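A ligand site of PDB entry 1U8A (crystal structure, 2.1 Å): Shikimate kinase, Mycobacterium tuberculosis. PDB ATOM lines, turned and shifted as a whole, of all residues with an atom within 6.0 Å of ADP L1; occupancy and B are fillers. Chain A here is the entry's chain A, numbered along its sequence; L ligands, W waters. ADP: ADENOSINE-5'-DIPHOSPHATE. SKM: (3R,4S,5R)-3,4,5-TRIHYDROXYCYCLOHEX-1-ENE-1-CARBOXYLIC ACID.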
ATOM      1  N   GLY A   9       9.595  14.065  30.352  1.00  0.00           N
ATOM      2  CA  GLY A   9      11.033  14.031  30.174  1.00  0.00           C
ATOM      3  C   GLY A   9      11.482  15.187  29.305  1.00  0.00           C
ATOM      4  O   GLY A   9      10.657  15.903  28.716  1.00  0.00           O
ATOM      5  N   LEU A  10      12.798  15.371  29.215  1.00  0.00           N
ATOM      6  CA  LEU A  10      13.383  16.448  28.431  1.00  0.00           C
ATOM      7  C   LEU A  10      13.112  16.255  26.956  1.00  0.00           C
ATOM      8  O   LEU A  10      12.669  15.194  26.525  1.00  0.00           O
ATOM      9  CB  LEU A  10      14.896  16.476  28.650  1.00  0.00           C
ATOM     10  CG  LEU A  10      15.436  16.828  30.036  1.00  0.00           C
ATOM     11  CD1 LEU A  10      16.905  16.453  30.133  1.00  0.00           C
ATOM     12  CD2 LEU A  10      15.265  18.322  30.273  1.00  0.00           C
ATOM     13  N   PRO A  11      13.343  17.302  26.155  1.00  0.00           N
ATOM     14  CA  PRO A  11      13.120  17.175  24.714  1.00  0.00           C
ATOM     15  C   PRO A  11      14.093  16.109  24.244  1.00  0.00           C
ATOM     16  O   PRO A  11      15.256  16.125  24.640  1.00  0.00           O
ATOM     17  CB  PRO A  11      13.519  18.543  24.194  1.00  0.00           C
ATOM     18  CG  PRO A  11      13.240  19.455  25.338  1.00  0.00           C
ATOM     19  CD  PRO A  11      13.741  18.671  26.511  1.00  0.00           C
ATOM     20  N   GLY A  12      13.625  15.182  23.407  1.00  0.00           N
ATOM     21  CA  GLY A  12      14.524  14.143  22.920  1.00  0.00           C
ATOM     22  C   GLY A  12      14.617  12.910  23.813  1.00  0.00           C
ATOM     23  O   GLY A  12      15.336  11.956  23.458  1.00  0.00           O
ATOM     24  N   SER A  13      13.939  12.906  24.949  1.00  0.00           N
ATOM     25  CA  SER A  13      13.993  11.740  25.829  1.00  0.00           C
ATOM     26  C   SER A  13      13.114  10.623  25.263  1.00  0.00           C
ATOM     27  O   SER A  13      13.253   9.478  25.653  1.00  0.00           O
ATOM     28  CB  SER A  13      13.551  12.105  27.264  1.00  0.00           C
ATOM     29  OG  SER A  13      12.196  12.484  27.346  1.00  0.00           O
ATOM     30  N   GLY A  14      12.218  10.976  24.349  1.00  0.00           N
ATOM     31  CA  GLY A  14      11.387   9.962  23.718  1.00  0.00           C
ATOM     32  C   GLY A  14       9.898   9.962  23.971  1.00  0.00           C
ATOM     33  O   GLY A  14       9.229   8.992  23.611  1.00  0.00           O
ATOM     34  N   LYS A  15       9.365  11.028  24.549  1.00  0.00           N
ATOM     35  CA  LYS A  15       7.931  11.122  24.834  1.00  0.00           C
ATOM     36  C   LYS A  15       7.036  10.770  23.644  1.00  0.00           C
ATOM     37  O   LYS A  15       6.158   9.927  23.728  1.00  0.00           O
ATOM     38  CB  LYS A  15       7.570  12.523  25.336  1.00  0.00           C
ATOM     39  CG  LYS A  15       8.324  12.956  26.594  1.00  0.00           C
ATOM     40  CD  LYS A  15       7.954  14.390  26.998  1.00  0.00           C
ATOM     41  CE  LYS A  15       8.510  15.430  26.010  1.00  0.00           C
ATOM     42  NZ  LYS A  15       9.980  15.575  26.135  1.00  0.00           N
ATOM     43  N   SER A  16       7.277  11.436  22.526  1.00  0.00           N
ATOM     44  CA  SER A  16       6.462  11.210  21.339  1.00  0.00           C
ATOM     45  C   SER A  16       6.659   9.826  20.711  1.00  0.00           C
ATOM     46  O   SER A  16       5.693   9.174  20.333  1.00  0.00           O
ATOM     47  CB  SER A  16       6.754  12.298  20.301  1.00  0.00           C
ATOM     48  OG  SER A  16       6.440  13.579  20.823  1.00  0.00           O
ATOM     49  N   THR A  17       7.911   9.385  20.629  1.00  0.00           N
ATOM     50  CA  THR A  17       8.236   8.089  20.038  1.00  0.00           C
ATOM     51  C   THR A  17       7.744   6.941  20.882  1.00  0.00           C
ATOM     52  O   THR A  17       6.984   6.087  20.413  1.00  0.00           O
ATOM     53  CB  THR A  17       9.754   7.930  19.854  1.00  0.00           C
ATOM     54  OG1 THR A  17      10.245   8.951  18.987  1.00  0.00           O
ATOM     55  CG2 THR A  17      10.089   6.553  19.256  1.00  0.00           C
ATOM     56  N   ILE A  18       8.165   6.920  22.143  1.00  0.00           N
ATOM     57  CA  ILE A  18       7.751   5.848  23.027  1.00  0.00           C
ATOM     58  C   ILE A  18       6.249   5.851  23.285  1.00  0.00           C
ATOM     59  O   ILE A  18       5.648   4.806  23.471  1.00  0.00           O
ATOM     60  CB  ILE A  18       8.542   5.919  24.338  1.00  0.00           C
ATOM     61  CG1 ILE A  18       9.986   5.539  24.046  1.00  0.00           C
ATOM     62  CG2 ILE A  18       7.956   4.987  25.375  1.00  0.00           C
ATOM     63  CD1 ILE A  18      10.894   5.696  25.211  1.00  0.00           C
ATOM     64  N   ASP A  32      -0.810  13.466  22.329  1.00  0.00           N
ATOM     65  CA  ASP A  32       0.416  14.225  22.514  1.00  0.00           C
ATOM     66  C   ASP A  32       0.005  15.666  22.716  1.00  0.00           C
ATOM     67  O   ASP A  32      -0.412  16.331  21.771  1.00  0.00           O
ATOM     68  CB  ASP A  32       1.303  14.100  21.273  1.00  0.00           C
ATOM     69  CG  ASP A  32       2.678  14.719  21.465  1.00  0.00           C
ATOM     70  OD1 ASP A  32       2.745  15.853  21.982  1.00  0.00           O
ATOM     71  OD2 ASP A  32       3.678  14.077  21.074  1.00  0.00           O
ATOM     72  N   LEU A 100      10.921   9.531  31.377  1.00  0.00           N
ATOM     73  CA  LEU A 100      11.948   8.991  30.486  1.00  0.00           C
ATOM     74  C   LEU A 100      13.260   9.748  30.696  1.00  0.00           C
ATOM     75  O   LEU A 100      13.402  10.897  30.269  1.00  0.00           O
ATOM     76  CB  LEU A 100      11.519   9.125  29.023  1.00  0.00           C
ATOM     77  CG  LEU A 100      10.248   8.357  28.640  1.00  0.00           C
ATOM     78  CD1 LEU A 100       9.846   8.694  27.201  1.00  0.00           C
ATOM     79  CD2 LEU A 100      10.515   6.866  28.787  1.00  0.00           C
ATOM     80  N   GLU A 106      23.538  12.229  25.038  1.00  0.00           N
ATOM     81  CA  GLU A 106      22.675  11.495  24.128  1.00  0.00           C
ATOM     82  C   GLU A 106      21.463  12.346  23.799  1.00  0.00           C
ATOM     83  O   GLU A 106      21.033  12.427  22.638  1.00  0.00           O
ATOM     84  CB  GLU A 106      22.253  10.180  24.786  1.00  0.00           C
ATOM     85  CG  GLU A 106      21.443   9.249  23.882  1.00  0.00           C
ATOM     86  CD  GLU A 106      22.068   9.046  22.508  1.00  0.00           C
ATOM     87  OE1 GLU A 106      23.305   8.879  22.429  1.00  0.00           O
ATOM     88  OE2 GLU A 106      21.321   9.053  21.506  1.00  0.00           O
ATOM     89  N   ARG A 110      20.161  13.426  20.098  1.00  0.00           N
ATOM     90  CA  ARG A 110      18.885  12.942  19.568  1.00  0.00           C
ATOM     91  C   ARG A 110      18.067  14.077  18.970  1.00  0.00           C
ATOM     92  O   ARG A 110      17.348  13.893  17.988  1.00  0.00           O
ATOM     93  CB  ARG A 110      18.057  12.247  20.656  1.00  0.00           C
ATOM     94  CG  ARG A 110      18.492  10.825  20.979  1.00  0.00           C
ATOM     95  CD  ARG A 110      17.482  10.218  21.933  1.00  0.00           C
ATOM     96  NE  ARG A 110      17.938   8.962  22.511  1.00  0.00           N
ATOM     97  CZ  ARG A 110      17.306   8.326  23.492  1.00  0.00           C
ATOM     98  NH1 ARG A 110      16.194   8.842  23.997  1.00  0.00           N
ATOM     99  NH2 ARG A 110      17.797   7.193  23.984  1.00  0.00           N
ATOM    100  N   THR A 111      18.183  15.267  19.575  1.00  0.00           N
ATOM    101  CA  THR A 111      17.438  16.426  19.112  1.00  0.00           C
ATOM    102  C   THR A 111      18.175  17.229  18.050  1.00  0.00           C
ATOM    103  O   THR A 111      17.800  18.364  17.759  1.00  0.00           O
ATOM    104  CB  THR A 111      17.119  17.375  20.289  1.00  0.00           C
ATOM    105  OG1 THR A 111      18.348  17.850  20.857  1.00  0.00           O
ATOM    106  CG2 THR A 111      16.318  16.649  21.364  1.00  0.00           C
ATOM    107  N   ARG A 117      12.259  22.726  18.247  1.00  0.00           N
ATOM    108  CA  ARG A 117      12.280  23.201  19.634  1.00  0.00           C
ATOM    109  C   ARG A 117      12.690  24.656  19.826  1.00  0.00           C
ATOM    110  O   ARG A 117      13.840  25.020  19.592  1.00  0.00           O
ATOM    111  CB  ARG A 117      13.270  22.345  20.444  1.00  0.00           C
ATOM    112  CG  ARG A 117      12.691  21.159  21.164  1.00  0.00           C
ATOM    113  CD  ARG A 117      11.722  20.362  20.313  1.00  0.00           C
ATOM    114  NE  ARG A 117      11.730  18.941  20.638  1.00  0.00           N
ATOM    115  CZ  ARG A 117      12.688  18.090  20.261  1.00  0.00           C
ATOM    116  NH1 ARG A 117      13.725  18.524  19.556  1.00  0.00           N
ATOM    117  NH2 ARG A 117      12.594  16.807  20.574  1.00  0.00           N
ATOM    118  N   THR A 150      16.529   5.617  29.623  1.00  0.00           N
ATOM    119  CA  THR A 150      16.510   5.294  28.199  1.00  0.00           C
ATOM    120  C   THR A 150      17.871   5.441  27.504  1.00  0.00           C
ATOM    121  O   THR A 150      17.941   5.418  26.276  1.00  0.00           O
ATOM    122  CB  THR A 150      15.534   6.192  27.415  1.00  0.00           C
ATOM    123  OG1 THR A 150      16.124   7.483  27.217  1.00  0.00           O
ATOM    124  CG2 THR A 150      14.227   6.336  28.175  1.00  0.00           C
ATOM    125  N   ASN A 151      18.933   5.583  28.288  1.00  0.00           N
ATOM    126  CA  ASN A 151      20.270   5.759  27.709  1.00  0.00           C
ATOM    127  C   ASN A 151      20.777   4.609  26.845  1.00  0.00           C
ATOM    128  O   ASN A 151      21.183   4.831  25.704  1.00  0.00           O
ATOM    129  CB  ASN A 151      21.279   6.093  28.811  1.00  0.00           C
ATOM    130  CG  ASN A 151      21.225   7.546  29.240  1.00  0.00           C
ATOM    131  OD1 ASN A 151      21.344   8.456  28.410  1.00  0.00           O
ATOM    132  ND2 ASN A 151      21.030   7.786  30.534  1.00  0.00           N
ATOM    133  N   ARG A 153      18.929   1.808  26.130  1.00  0.00           N
ATOM    134  CA  ARG A 153      17.778   1.023  25.704  1.00  0.00           C
ATOM    135  C   ARG A 153      17.193   1.555  24.402  1.00  0.00           C
ATOM    136  O   ARG A 153      16.930   2.755  24.272  1.00  0.00           O
ATOM    137  CB  ARG A 153      16.653   1.076  26.761  1.00  0.00           C
ATOM    138  CG  ARG A 153      16.953   0.453  28.132  1.00  0.00           C
ATOM    139  CD  ARG A 153      15.644   0.297  28.919  1.00  0.00           C
ATOM    140  NE  ARG A 153      15.761  -0.557  30.116  1.00  0.00           N
ATOM    141  CZ  ARG A 153      15.960  -0.105  31.353  1.00  0.00           C
ATOM    142  NH1 ARG A 153      16.081   1.197  31.588  1.00  0.00           N
ATOM    143  NH2 ARG A 153      16.042  -0.960  32.365  1.00  0.00           N
ATOM    144  N   ASN A 154      16.985   0.669  23.436  1.00  0.00           N
ATOM    145  CA  ASN A 154      16.370   1.075  22.169  1.00  0.00           C
ATOM    146  C   ASN A 154      14.871   1.258  22.509  1.00  0.00           C
ATOM    147  O   ASN A 154      14.406   0.807  23.545  1.00  0.00           O
ATOM    148  CB  ASN A 154      16.591  -0.002  21.101  1.00  0.00           C
ATOM    149  CG  ASN A 154      16.205  -1.386  21.573  1.00  0.00           C
ATOM    150  OD1 ASN A 154      15.028  -1.702  21.712  1.00  0.00           O
ATOM    151  ND2 ASN A 154      17.214  -2.217  21.839  1.00  0.00           N
ATOM    152  N   PRO A 155      14.097   1.916  21.630  1.00  0.00           N
ATOM    153  CA  PRO A 155      12.674   2.130  21.896  1.00  0.00           C
ATOM    154  C   PRO A 155      11.865   0.916  22.331  1.00  0.00           C
ATOM    155  O   PRO A 155      11.137   0.968  23.326  1.00  0.00           O
ATOM    156  CB  PRO A 155      12.164   2.731  20.584  1.00  0.00           C
ATOM    157  CG  PRO A 155      13.369   3.492  20.092  1.00  0.00           C
ATOM    158  CD  PRO A 155      14.496   2.508  20.346  1.00  0.00           C
ATOM    159  N   VAL A 158      12.482   0.074  25.870  1.00  0.00           N
ATOM    160  CA  VAL A 158      11.868   1.017  26.797  1.00  0.00           C
ATOM    161  C   VAL A 158      10.373   0.700  26.883  1.00  0.00           C
ATOM    162  O   VAL A 158       9.821   0.622  27.971  1.00  0.00           O
ATOM    163  CB  VAL A 158      12.053   2.477  26.355  1.00  0.00           C
ATOM    164  CG1 VAL A 158      11.313   3.405  27.313  1.00  0.00           C
ATOM    165  CG2 VAL A 158      13.548   2.831  26.333  1.00  0.00           C
HETATM  166  PB  ADP L   1      10.408  13.940  22.700  1.00  0.00           P
HETATM  167  O1B ADP L   1      10.597  13.589  24.123  1.00  0.00           O
HETATM  168  O2B ADP L   1      10.845  15.296  22.148  1.00  0.00           O
HETATM  169  O3B ADP L   1       8.899  13.568  22.183  1.00  0.00           O
HETATM  170  PA  ADP L   1      10.937  12.170  20.507  1.00  0.00           P
HETATM  171  O1A ADP L   1       9.972  11.063  20.818  1.00  0.00           O
HETATM  172  O2A ADP L   1      10.588  13.155  19.413  1.00  0.00           O
HETATM  173  O3A ADP L   1      11.269  12.977  21.808  1.00  0.00           O
HETATM  174  O5' ADP L   1      12.380  11.486  20.228  1.00  0.00           O
HETATM  175  C5' ADP L   1      13.442  12.327  19.605  1.00  0.00           C
HETATM  176  C4' ADP L   1      14.309  11.426  18.681  1.00  0.00           C
HETATM  177  O4' ADP L   1      15.001  10.390  19.431  1.00  0.00           O
HETATM  178  C3' ADP L   1      13.538  10.616  17.618  1.00  0.00           C
HETATM  179  O3' ADP L   1      14.130  10.729  16.285  1.00  0.00           O
HETATM  180  C2' ADP L   1      13.538   9.160  18.071  1.00  0.00           C
HETATM  181  O2' ADP L   1      13.532   8.214  16.988  1.00  0.00           O
HETATM  182  C1' ADP L   1      14.761   9.045  18.896  1.00  0.00           C
HETATM  183  N9  ADP L   1      14.731   8.174  20.130  1.00  0.00           N
HETATM  184  C8  ADP L   1      13.775   8.271  21.165  1.00  0.00           C
HETATM  185  N7  ADP L   1      13.864   7.235  21.986  1.00  0.00           N
HETATM  186  C5  ADP L   1      15.013   6.560  21.615  1.00  0.00           C
HETATM  187  C6  ADP L   1      15.702   5.419  22.167  1.00  0.00           C
HETATM  188  N6  ADP L   1      15.255   4.687  23.195  1.00  0.00           N
HETATM  189  N1  ADP L   1      16.916   5.043  21.558  1.00  0.00           N
HETATM  190  C2  ADP L   1      17.256   5.609  20.331  1.00  0.00           C
HETATM  191  N3  ADP L   1      16.720   6.739  19.751  1.00  0.00           N
HETATM  192  C4  ADP L   1      15.563   7.138  20.465  1.00  0.00           C
HETATM  193  O12 SKM L   2       6.252  21.411  24.236  1.00  0.00           O
HETATM  194  C8  SKM L   2       7.197  21.616  23.181  1.00  0.00           C
HETATM  195  C6  SKM L   2       7.678  23.075  23.219  1.00  0.00           C
HETATM  196  O7  SKM L   2       8.670  23.292  22.221  1.00  0.00           O
HETATM  197  C5  SKM L   2       8.238  23.392  24.616  1.00  0.00           C
HETATM  198  C4  SKM L   2       9.196  22.299  25.132  1.00  0.00           C
HETATM  199  C1  SKM L   2      10.048  22.577  26.386  1.00  0.00           C
HETATM  200  O2  SKM L   2       9.782  23.598  27.131  1.00  0.00           O
HETATM  201  O3  SKM L   2      11.002  21.777  26.722  1.00  0.00           O
HETATM  202  C10 SKM L   2       9.263  21.079  24.570  1.00  0.00           C
HETATM  203  C9  SKM L   2       8.393  20.659  23.364  1.00  0.00           C
HETATM  204  O11 SKM L   2       7.931  19.322  23.549  1.00  0.00           O
HETATM  205  O   HOH W   1      13.458   6.599  24.687  1.00  0.00           O
HETATM  206  O   HOH W   2       9.902  17.352  24.168  1.00  0.00           O
HETATM  207  O   HOH W   3       8.744  12.288  17.505  1.00  0.00           O
HETATM  208  O   HOH W   4       8.882  14.985  19.946  1.00  0.00           O
HETATM  209  O   HOH W   5      14.425  15.021  17.855  1.00  0.00           O
HETATM  210  O   HOH W   6      13.771   5.705  17.763  1.00  0.00           O
HETATM  211  O   HOH W   7       9.498  17.803  21.276  1.00  0.00           O
HETATM  212  O   HOH W   8       6.892  15.903  22.224  1.00  0.00           O
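The side-chain hydroxyl (OG) of Ser 16 lies within hydrogen-bond range of the side-chain carboxylate (OD2) of Asp 32, 2.8 Å away.
The side-chain amino group (NZ) of Lys 15 is in hydrogen-bond range of the backbone carbonyl oxygen (O) of Leu 10, 2.7 Å away.
The side-chain amino group (NZ) of Lys 15 sits at hydrogen-bond distance from the backbone carbonyl oxygen (O) of Gly 9 (2.7 Å).
The backbone carbonyl oxygen of Gly 12 lies close to the guanidinium group of Arg 110, at 3.3 Å.
The backbone carbonyl oxygen (O) of Ser 13 sits at hydrogen-bond distance from the guanidinium group (NH1) of Arg 110 (3.4 Å).
NH2 of Arg 110 is in hydrogen-bond range of O of Thr 150 (2.9 Å).
The guanidinium group (NE) of Arg 110 is in salt-bridge range of the side-chain carboxylate (OE2) of Glu 106, at 3.5 Å.
O of Leu 10 sits at hydrogen-bond distance from OG of Ser 13.
Water W4 bridges an oxygen (O2A) of ADP L1 (2.6 Å) and the side-chain hydroxyl (OG) of Ser 16 (3.0 Å).
Water W1 lies within hydrogen-bond range of N7 of ADP L1 (2.8 Å) and O of Ser 13 (3.0 Å).
Water W7 lies within hydrogen-bond range of the guanidinium group (NE) of Arg 117, an oxygen (O2B) of ADP L1 and an oxygen (O11) of SKM L2.
Water W2 lies within hydrogen-bond range of the side-chain amino group (NZ) of Lys 15 (2.7 Å), an oxygen (O11) of SKM L2 (2.9 Å) and an oxygen (O2B) of ADP L1 (3.0 Å).
Water W8 lies within hydrogen-bond range of OG of Ser 16 (2.8 Å) and O3B of ADP L1 (3.1 Å).
A nitrogen (N6) of ADP L1 sits close to the backbone nitrogen (N) of Pro 155 (3.4 Å).
Leu 10 touches ADP L1.
CA of Pro 11 touches O2B of ADP L1 (3.9 Å).
Ser 13 touches ADP L1 (N to O1B, 3.5 Å).
Asn 154 touches ADP L1.
The nearest printed residue that does not touch ADP L1 is Val 158 (4.03 Å).
O1A of ADP L1 is in hydrogen-bond range of N of Thr 17, at 2.7 Å.
O1A of ADP L1 is in hydrogen-bond range of OG1 of Thr 17 (2.8 Å).
N of Ser 16 sits at hydrogen-bond distance from O3B of ADP L1 (2.7 Å).
The side-chain hydroxyl of Ser 16 sits at hydrogen-bond distance from an oxygen (O3B) of ADP L1 (2.8 Å).
A nitrogen (N6) of ADP L1 sits at hydrogen-bond distance from the backbone carbonyl oxygen of Arg 153, at 2.8 Å.
NH2 of Arg 117 is in salt-bridge range of O2B of ADP L1 (2.8 Å).
O1B of ADP L1 is in hydrogen-bond range of N of Lys 15, 2.9 Å away.
The side-chain amino group (NZ) of Lys 15 is in salt-bridge range of an oxygen (O1B) of ADP L1, 2.9 Å away.
The backbone NH (N) of Gly 12 is in hydrogen-bond range of an oxygen (O2B) of ADP L1 (3.1 Å).
An oxygen (O1B) of ADP L1 is in hydrogen-bond range of the backbone NH (N) of Gly 14.
NH2 of Arg 110 lies close to N1 of ADP L1.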
